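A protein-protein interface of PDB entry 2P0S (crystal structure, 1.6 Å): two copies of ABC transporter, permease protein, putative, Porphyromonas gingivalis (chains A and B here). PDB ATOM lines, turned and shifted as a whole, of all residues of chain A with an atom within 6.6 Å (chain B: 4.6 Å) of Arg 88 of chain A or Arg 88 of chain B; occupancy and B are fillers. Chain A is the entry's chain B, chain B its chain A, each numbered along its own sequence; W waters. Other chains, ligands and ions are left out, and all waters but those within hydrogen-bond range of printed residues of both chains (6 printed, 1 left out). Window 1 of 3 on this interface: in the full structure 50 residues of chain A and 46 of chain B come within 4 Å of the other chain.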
ATOM      1  N   LEU A  24     -17.552   4.042  24.174  1.00  0.00           N
ATOM      2  CA  LEU A  24     -18.843   3.720  24.729  1.00  0.00           C
ATOM      3  C   LEU A  24     -18.951   2.239  25.040  1.00  0.00           C
ATOM      4  O   LEU A  24     -19.907   1.892  25.695  1.00  0.00           O
ATOM      5  CB  LEU A  24     -19.907   4.010  23.666  1.00  0.00           C
ATOM      6  CG  LEU A  24     -20.138   5.465  23.285  1.00  0.00           C
ATOM      7  CD1 LEU A  24     -21.203   5.555  22.139  1.00  0.00           C
ATOM      8  CD2 LEU A  24     -20.562   6.319  24.513  1.00  0.00           C
ATOM      9  N   SER A  83     -25.923  -7.475  17.729  1.00  0.00           N
ATOM     10  CA  SER A  83     -26.243  -6.179  17.140  1.00  0.00           C
ATOM     11  C   SER A  83     -27.243  -5.461  17.989  1.00  0.00           C
ATOM     12  O   SER A  83     -27.240  -4.198  17.987  1.00  0.00           O
ATOM     13  CB  SER A  83     -26.784  -6.267  15.750  1.00  0.00           C
ATOM     14  OG  SER A  83     -27.547  -7.452  15.705  1.00  0.00           O
ATOM     15  N   ASN A  84     -28.157  -6.195  18.705  1.00  0.00           N
ATOM     16  CA  ASN A  84     -29.101  -5.450  19.596  1.00  0.00           C
ATOM     17  C   ASN A  84     -28.324  -4.676  20.621  1.00  0.00           C
ATOM     18  O   ASN A  84     -28.617  -3.456  20.835  1.00  0.00           O
ATOM     19  CB  ASN A  84     -30.114  -6.266  20.344  1.00  0.00           C
ATOM     20  CG  ASN A  84     -31.080  -6.922  19.396  1.00  0.00           C
ATOM     21  OD1 ASN A  84     -31.252  -6.479  18.246  1.00  0.00           O
ATOM     22  ND2 ASN A  84     -31.738  -7.969  19.872  1.00  0.00           N
ATOM     23  N   HIS A  85     -27.310  -5.293  21.232  1.00  0.00           N
ATOM     24  CA  HIS A  85     -26.542  -4.551  22.309  1.00  0.00           C
ATOM     25  C   HIS A  85     -25.811  -3.420  21.688  1.00  0.00           C
ATOM     26  O   HIS A  85     -25.883  -2.317  22.229  1.00  0.00           O
ATOM     27  CB  HIS A  85     -25.494  -5.535  22.935  1.00  0.00           C
ATOM     28  CG  HIS A  85     -24.673  -4.926  24.056  1.00  0.00           C
ATOM     29  ND1 HIS A  85     -25.273  -4.441  25.199  1.00  0.00           N
ATOM     30  CD2 HIS A  85     -23.335  -4.789  24.240  1.00  0.00           C
ATOM     31  CE1 HIS A  85     -24.345  -3.970  26.025  1.00  0.00           C
ATOM     32  NE2 HIS A  85     -23.155  -4.221  25.492  1.00  0.00           N
ATOM     33  N   ILE A  86     -25.156  -3.646  20.539  1.00  0.00           N
ATOM     34  CA  ILE A  86     -24.312  -2.526  19.982  1.00  0.00           C
ATOM     35  C   ILE A  86     -25.251  -1.409  19.514  1.00  0.00           C
ATOM     36  O   ILE A  86     -24.988  -0.166  19.648  1.00  0.00           O
ATOM     37  CB  ILE A  86     -23.485  -3.077  18.778  1.00  0.00           C
ATOM     38  CG1 ILE A  86     -22.349  -3.992  19.343  1.00  0.00           C
ATOM     39  CG2 ILE A  86     -22.962  -1.934  17.852  1.00  0.00           C
ATOM     40  CD1 ILE A  86     -21.628  -4.832  18.308  1.00  0.00           C
ATOM     41  N   SER A  87     -26.305  -1.795  18.823  1.00  0.00           N
ATOM     42  CA  SER A  87     -27.247  -0.783  18.370  1.00  0.00           C
ATOM     43  C   SER A  87     -27.830   0.042  19.484  1.00  0.00           C
ATOM     44  O   SER A  87     -28.047   1.252  19.271  1.00  0.00           O
ATOM     45  CB  SER A  87     -28.392  -1.414  17.670  1.00  0.00           C
ATOM     46  OG  SER A  87     -27.949  -2.149  16.463  1.00  0.00           O
ATOM     47  N   ARG A  88     -28.173  -0.569  20.643  1.00  0.00           N
ATOM     48  CA  ARG A  88     -28.750   0.222  21.708  1.00  0.00           C
ATOM     49  C   ARG A  88     -27.661   1.173  22.275  1.00  0.00           C
ATOM     50  O   ARG A  88     -28.008   2.343  22.537  1.00  0.00           O
ATOM     51  CB  ARG A  88     -29.248  -0.710  22.808  1.00  0.00           C
ATOM     52  CG  ARG A  88     -29.653   0.040  24.062  1.00  0.00           C
ATOM     53  CD  ARG A  88     -31.128   0.050  24.184  1.00  0.00           C
ATOM     54  NE  ARG A  88     -31.598   1.220  24.923  1.00  0.00           N
ATOM     55  CZ  ARG A  88     -32.894   1.483  25.151  1.00  0.00           C
ATOM     56  NH1 ARG A  88     -33.862   0.634  24.718  1.00  0.00           N
ATOM     57  NH2 ARG A  88     -33.217   2.595  25.847  1.00  0.00           N
ATOM     58  N   ILE A  89     -26.410   0.705  22.432  1.00  0.00           N
ATOM     59  CA  ILE A  89     -25.335   1.594  22.894  1.00  0.00           C
ATOM     60  C   ILE A  89     -25.194   2.833  21.950  1.00  0.00           C
ATOM     61  O   ILE A  89     -25.149   3.978  22.419  1.00  0.00           O
ATOM     62  CB  ILE A  89     -23.972   0.884  22.935  1.00  0.00           C
ATOM     63  CG1 ILE A  89     -23.960  -0.047  24.157  1.00  0.00           C
ATOM     64  CG2 ILE A  89     -22.786   1.890  23.111  1.00  0.00           C
ATOM     65  CD1 ILE A  89     -22.732  -0.895  24.181  1.00  0.00           C
ATOM     66  N   LEU A  90     -25.102   2.594  20.655  1.00  0.00           N
ATOM     67  CA  LEU A  90     -25.019   3.702  19.695  1.00  0.00           C
ATOM     68  C   LEU A  90     -26.283   4.564  19.714  1.00  0.00           C
ATOM     69  O   LEU A  90     -26.215   5.817  19.659  1.00  0.00           O
ATOM     70  CB  LEU A  90     -24.733   3.179  18.288  1.00  0.00           C
ATOM     71  CG  LEU A  90     -23.342   2.504  18.153  1.00  0.00           C
ATOM     72  CD1 LEU A  90     -23.282   1.905  16.707  1.00  0.00           C
ATOM     73  CD2 LEU A  90     -22.126   3.564  18.293  1.00  0.00           C
ATOM     74  N   SER A  91     -27.462   3.956  19.666  1.00  0.00           N
ATOM     75  CA  SER A  91     -28.735   4.733  19.621  1.00  0.00           C
ATOM     76  C   SER A  91     -28.809   5.651  20.872  1.00  0.00           C
ATOM     77  O   SER A  91     -29.290   6.763  20.709  1.00  0.00           O
ATOM     78  CB  SER A  91     -29.962   3.813  19.634  1.00  0.00           C
ATOM     79  OG  SER A  91     -29.936   3.165  18.330  1.00  0.00           O
ATOM     80  N   ASP A  92     -28.517   5.122  22.095  1.00  0.00           N
ATOM     81  CA  ASP A  92     -28.613   6.010  23.322  1.00  0.00           C
ATOM     82  C   ASP A  92     -27.718   7.198  23.122  1.00  0.00           C
ATOM     83  O   ASP A  92     -28.107   8.364  23.510  1.00  0.00           O
ATOM     84  CB  ASP A  92     -28.189   5.174  24.572  1.00  0.00           C
ATOM     85  CG  ASP A  92     -29.423   4.354  25.113  1.00  0.00           C
ATOM     86  OD1 ASP A  92     -30.568   4.527  24.548  1.00  0.00           O
ATOM     87  OD2 ASP A  92     -29.276   3.554  26.062  1.00  0.00           O
ATOM     88  N   TYR A  93     -26.513   6.955  22.656  1.00  0.00           N
ATOM     89  CA  TYR A  93     -25.493   8.057  22.541  1.00  0.00           C
ATOM     90  C   TYR A  93     -25.967   9.078  21.493  1.00  0.00           C
ATOM     91  O   TYR A  93     -25.928  10.331  21.675  1.00  0.00           O
ATOM     92  CB  TYR A  93     -24.123   7.522  22.090  1.00  0.00           C
ATOM     93  CG  TYR A  93     -23.111   8.678  21.902  1.00  0.00           C
ATOM     94  CD1 TYR A  93     -22.528   9.279  23.026  1.00  0.00           C
ATOM     95  CD2 TYR A  93     -22.746   9.165  20.641  1.00  0.00           C
ATOM     96  CE1 TYR A  93     -21.582  10.319  22.829  1.00  0.00           C
ATOM     97  CE2 TYR A  93     -21.835  10.165  20.435  1.00  0.00           C
ATOM     98  CZ  TYR A  93     -21.270  10.746  21.550  1.00  0.00           C
ATOM     99  OH  TYR A  93     -20.382  11.776  21.384  1.00  0.00           O
ATOM    100  N   LEU A 118     -28.824   4.306  35.513  1.00  0.00           N
ATOM    101  CA  LEU A 118     -28.921   3.189  36.437  1.00  0.00           C
ATOM    102  C   LEU A 118     -28.092   2.065  35.880  1.00  0.00           C
ATOM    103  O   LEU A 118     -27.990   1.857  34.679  1.00  0.00           O
ATOM    104  CB  LEU A 118     -30.379   2.644  36.564  1.00  0.00           C
ATOM    105  CG  LEU A 118     -31.505   3.606  36.889  1.00  0.00           C
ATOM    106  CD1 LEU A 118     -32.815   2.815  36.967  1.00  0.00           C
ATOM    107  CD2 LEU A 118     -31.310   4.408  38.182  1.00  0.00           C
ATOM    108  N   VAL A 120     -28.889  -1.462  37.140  1.00  0.00           N
ATOM    109  CA  VAL A 120     -29.681  -2.352  37.963  1.00  0.00           C
ATOM    110  C   VAL A 120     -28.908  -3.656  38.355  1.00  0.00           C
ATOM    111  O   VAL A 120     -28.419  -4.385  37.439  1.00  0.00           O
ATOM    112  CB  VAL A 120     -30.983  -2.727  37.216  1.00  0.00           C
ATOM    113  CG1 VAL A 120     -31.781  -3.775  38.074  1.00  0.00           C
ATOM    114  CG2 VAL A 120     -31.832  -1.468  36.910  1.00  0.00           C
ATOM    115  N   ASN B  84     -28.355  -4.649  31.518  1.00  0.00           N
ATOM    116  CA  ASN B  84     -27.945  -3.588  30.552  1.00  0.00           C
ATOM    117  C   ASN B  84     -29.172  -2.908  29.991  1.00  0.00           C
ATOM    118  O   ASN B  84     -29.431  -1.693  30.262  1.00  0.00           O
ATOM    119  CB  ASN B  84     -27.070  -4.153  29.410  1.00  0.00           C
ATOM    120  CG  ASN B  84     -25.680  -4.506  29.884  1.00  0.00           C
ATOM    121  OD1 ASN B  84     -24.897  -5.175  29.173  1.00  0.00           O
ATOM    122  ND2 ASN B  84     -25.344  -4.039  31.099  1.00  0.00           N
ATOM    123  N   HIS B  85     -29.959  -3.724  29.315  1.00  0.00           N
ATOM    124  CA  HIS B  85     -31.135  -3.350  28.479  1.00  0.00           C
ATOM    125  C   HIS B  85     -32.203  -2.703  29.354  1.00  0.00           C
ATOM    126  O   HIS B  85     -32.678  -1.590  29.052  1.00  0.00           O
ATOM    127  CB  HIS B  85     -31.719  -4.654  27.891  1.00  0.00           C
ATOM    128  CG  HIS B  85     -32.863  -4.459  26.924  1.00  0.00           C
ATOM    129  ND1 HIS B  85     -32.734  -3.768  25.728  1.00  0.00           N
ATOM    130  CD2 HIS B  85     -34.143  -4.919  26.944  1.00  0.00           C
ATOM    131  CE1 HIS B  85     -33.885  -3.796  25.066  1.00  0.00           C
ATOM    132  NE2 HIS B  85     -34.743  -4.503  25.772  1.00  0.00           N
ATOM    133  N   ILE B  86     -32.524  -3.337  30.476  1.00  0.00           N
ATOM    134  CA  ILE B  86     -33.538  -2.875  31.395  1.00  0.00           C
ATOM    135  C   ILE B  86     -33.071  -1.545  32.004  1.00  0.00           C
ATOM    136  O   ILE B  86     -33.866  -0.599  32.071  1.00  0.00           O
ATOM    137  CB  ILE B  86     -33.802  -3.888  32.454  1.00  0.00           C
ATOM    138  CG1 ILE B  86     -34.533  -5.113  31.758  1.00  0.00           C
ATOM    139  CG2 ILE B  86     -34.599  -3.308  33.572  1.00  0.00           C
ATOM    140  CD1 ILE B  86     -34.818  -6.282  32.731  1.00  0.00           C
ATOM    141  N   SER B  87     -31.821  -1.461  32.384  1.00  0.00           N
ATOM    142  CA  SER B  87     -31.286  -0.196  33.035  1.00  0.00           C
ATOM    143  C   SER B  87     -31.379   1.010  32.080  1.00  0.00           C
ATOM    144  O   SER B  87     -31.750   2.122  32.486  1.00  0.00           O
ATOM    145  CB  SER B  87     -29.815  -0.414  33.383  1.00  0.00           C
ATOM    146  OG  SER B  87     -29.673  -1.431  34.408  1.00  0.00           O
ATOM    147  N   ARG B  88     -31.064   0.753  30.807  1.00  0.00           N
ATOM    148  CA  ARG B  88     -31.129   1.857  29.784  1.00  0.00           C
ATOM    149  C   ARG B  88     -32.559   2.286  29.501  1.00  0.00           C
ATOM    150  O   ARG B  88     -32.846   3.474  29.296  1.00  0.00           O
ATOM    151  CB  ARG B  88     -30.460   1.495  28.484  1.00  0.00           C
ATOM    152  CG  ARG B  88     -28.905   1.412  28.519  1.00  0.00           C
ATOM    153  CD  ARG B  88     -28.271   0.818  27.182  1.00  0.00           C
ATOM    154  NE  ARG B  88     -26.837   0.683  27.382  1.00  0.00           N
ATOM    155  CZ  ARG B  88     -26.035   1.715  27.124  1.00  0.00           C
ATOM    156  NH1 ARG B  88     -26.565   2.837  26.647  1.00  0.00           N
ATOM    157  NH2 ARG B  88     -24.693   1.598  27.343  1.00  0.00           N
ATOM    158  N   ILE B  89     -33.501   1.340  29.477  1.00  0.00           N
ATOM    159  CA  ILE B  89     -34.892   1.657  29.194  1.00  0.00           C
ATOM    160  C   ILE B  89     -35.376   2.552  30.374  1.00  0.00           C
ATOM    161  O   ILE B  89     -35.955   3.596  30.137  1.00  0.00           O
ATOM    162  CB  ILE B  89     -35.774   0.351  29.022  1.00  0.00           C
ATOM    163  CG1 ILE B  89     -35.468  -0.311  27.681  1.00  0.00           C
ATOM    164  CG2 ILE B  89     -37.241   0.599  29.066  1.00  0.00           C
ATOM    165  CD1 ILE B  89     -35.992  -1.727  27.679  1.00  0.00           C
ATOM    166  N   LEU B  90     -35.086   2.163  31.644  1.00  0.00           N
ATOM    167  CA  LEU B  90     -35.593   2.860  32.799  1.00  0.00           C
ATOM    168  C   LEU B  90     -34.890   4.211  32.779  1.00  0.00           C
ATOM    169  O   LEU B  90     -35.515   5.270  33.050  1.00  0.00           O
ATOM    170  CB  LEU B  90     -35.239   2.097  34.090  1.00  0.00           C
ATOM    171  CG  LEU B  90     -36.091   0.844  34.282  1.00  0.00           C
ATOM    172  CD1 LEU B  90     -35.531   0.125  35.537  1.00  0.00           C
ATOM    173  CD2 LEU B  90     -37.577   1.270  34.581  1.00  0.00           C
ATOM    174  N   SER B  91     -33.600   4.188  32.481  1.00  0.00           N
ATOM    175  CA  SER B  91     -32.778   5.489  32.563  1.00  0.00           C
ATOM    176  C   SER B  91     -33.234   6.535  31.586  1.00  0.00           C
ATOM    177  O   SER B  91     -33.270   7.764  31.849  1.00  0.00           O
ATOM    178  CB  SER B  91     -31.266   5.245  32.313  1.00  0.00           C
ATOM    179  OG  SER B  91     -30.724   4.277  33.255  1.00  0.00           O
ATOM    180  N   ASP B  92     -33.627   6.046  30.415  1.00  0.00           N
ATOM    181  CA  ASP B  92     -33.971   7.012  29.351  1.00  0.00           C
ATOM    182  C   ASP B  92     -35.325   7.587  29.743  1.00  0.00           C
ATOM    183  O   ASP B  92     -35.612   8.782  29.498  1.00  0.00           O
ATOM    184  CB  ASP B  92     -34.105   6.269  28.018  1.00  0.00           C
ATOM    185  CG  ASP B  92     -32.779   5.846  27.342  1.00  0.00           C
ATOM    186  OD1 ASP B  92     -31.681   6.386  27.643  1.00  0.00           O
ATOM    187  OD2 ASP B  92     -32.900   4.959  26.393  1.00  0.00           O
HETATM  188  O   HOH W   1     -29.601   4.814  28.203  1.00  0.00           O
HETATM  189  O   HOH W   2     -28.154   2.691  32.045  1.00  0.00           O
HETATM  190  O   HOH W   3     -30.641   8.412  25.340  1.00  0.00           O
HETATM  191  O   HOH W   4     -32.422   6.660  23.497  1.00  0.00           O
HETATM  192  O   HOH W   5     -24.628   4.694  25.190  1.00  0.00           O
HETATM  193  O   HOH W   6     -22.161   3.302  26.566  1.00  0.00           O
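The side-chain hydroxyl of Ser 91 of chain B is in hydrogen-bond range of the backbone NH of Leu 118 of chain A, 3.0 Å away. OG of Ser 87 of chain B sits at hydrogen-bond distance from N of Val 120 of chain A, 2.8 Å away. OD2 of Asp 92 of chain B sits close to OD1 of Asp 92 of chain A, 3.0 Å away. The side-chain carboxylate (OD2) of Asp 92 of chain A lies within salt-bridge range of the guanidinium group (NH1) of Arg 88 of chain B, 2.9 Å away. The side-chain carboxylate (OD2) of Asp 92 of chain B lies within salt-bridge range of the guanidinium group (NH2) of Arg 88 of chain A, at 2.4 Å.
The backbone carbonyl oxygen of Ser 87 of chain B is in hydrogen-bond range of the side-chain hydroxyl of Ser 91 of chain B (2.5 Å). NE of Arg 88 of chain A is in salt-bridge range of OD2 of Asp 92 of chain A (3.5 Å).
Among the printed residues, pairs that only touch across the chains: Leu 118 of chain A with Ser 87 of chain B, His 85 of chain A with Asn 84 of chain B, Arg 88 of chain A with Arg 88 of chain B, Arg 88 of chain A with Ile 89 of chain B, Ile 89 of chain A with Arg 88 of chain B and Leu 118 of chain A with Leu 90 of chain B.
Printed residues of chain B within 4 Å of His 85 of chain A: Asn 84 (3.4 Å). Printed residues of chain B within 4 Å of Leu 118 of chain A: Ser 87 (3.2 Å), Leu 90 (3.8 Å) and Ser 91 (3.0 Å). Printed residues of chain B within 4 Å of Val 120 of chain A: Ser 87 (2.8 Å). Of the printed residues of chain A, Asn 84 of chain B touches His 85 (3.4 Å). Of chain A, only Arg 88 (3.5 Å), Ile 89 (3.7 Å) and Asp 92 (2.9 Å) come within 4 Å of Arg 88 of chain B. The nearest printed residue of chain A that does not touch Arg 88 of chain B is Leu 118 of chain A (5.1 Å). The nearest printed residue of chain B that does not touch Leu 118 of chain A is Arg 88 of chain B (5.1 Å).
Of the 14 printed residues of chain A, 6 touch a printed residue of chain B. Hydrophobic or aromatic side chains of chain B within 4 Å of the printed part of chain A: Ile 89 and Leu 90. Among the printed residues, 11 pairs touch across the chains. Among the printed residues, Asp or Glu carboxylates within 4 Å of a Lys or Arg side-chain nitrogen of the other chain: Arg 88 of chain A with Asp 92 of chain B (2.4 Å) and Asp 92 of chain A with Arg 88 of chain B (2.9 Å).
His 85 of chain A touches Asn 84 of chain B, but with the chains exchanged Asn 84 of chain A does not touch His 85 of chain B (6.4 Å). Arg 88 of chain A touches Ile 89 of chain B, and with the chains exchanged Ile 89 of chain A touches Arg 88 of chain B. Arg 88 of chain A touches Asp 92 of chain B, and with the chains exchanged Asp 92 of chain A touches Arg 88 of chain B. Asp 92 of chain A touches its own counterpart, Asp 92 of chain B. 9 positions are printed for both chains. Of the 11 pairs that touch across the chains among the printed residues, 6 have their exchanged pair printed and touching as well.
Water W1 lies within hydrogen-bond range of the side-chain carboxylate (OD2) of Asp 92 of chain A (2.5 Å) and the side-chain carboxylate (OD1) of Asp 92 of chain B (2.7 Å). Water W2 lies within hydrogen-bond range of O of Leu 118 of chain A (2.8 Å) and OG of Ser 91 of chain B (3.3 Å). Water W6 lies within hydrogen-bond range of O of Leu 24 of chain A (2.8 Å) and NH2 of Arg 88 of chain B (3.1 Å). Water W5 lies within hydrogen-bond range of O of Ile 89 of chain A (2.9 Å) and NH1 of Arg 88 of chain B (3.1 Å). Water W4 lies within hydrogen-bond range of OD1 of Asp 92 of chain A and OD2 of Asp 92 of chain B. Water W3 bridges O of Asp 92 of chain A and OD1 of Asp 92 of chain B.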
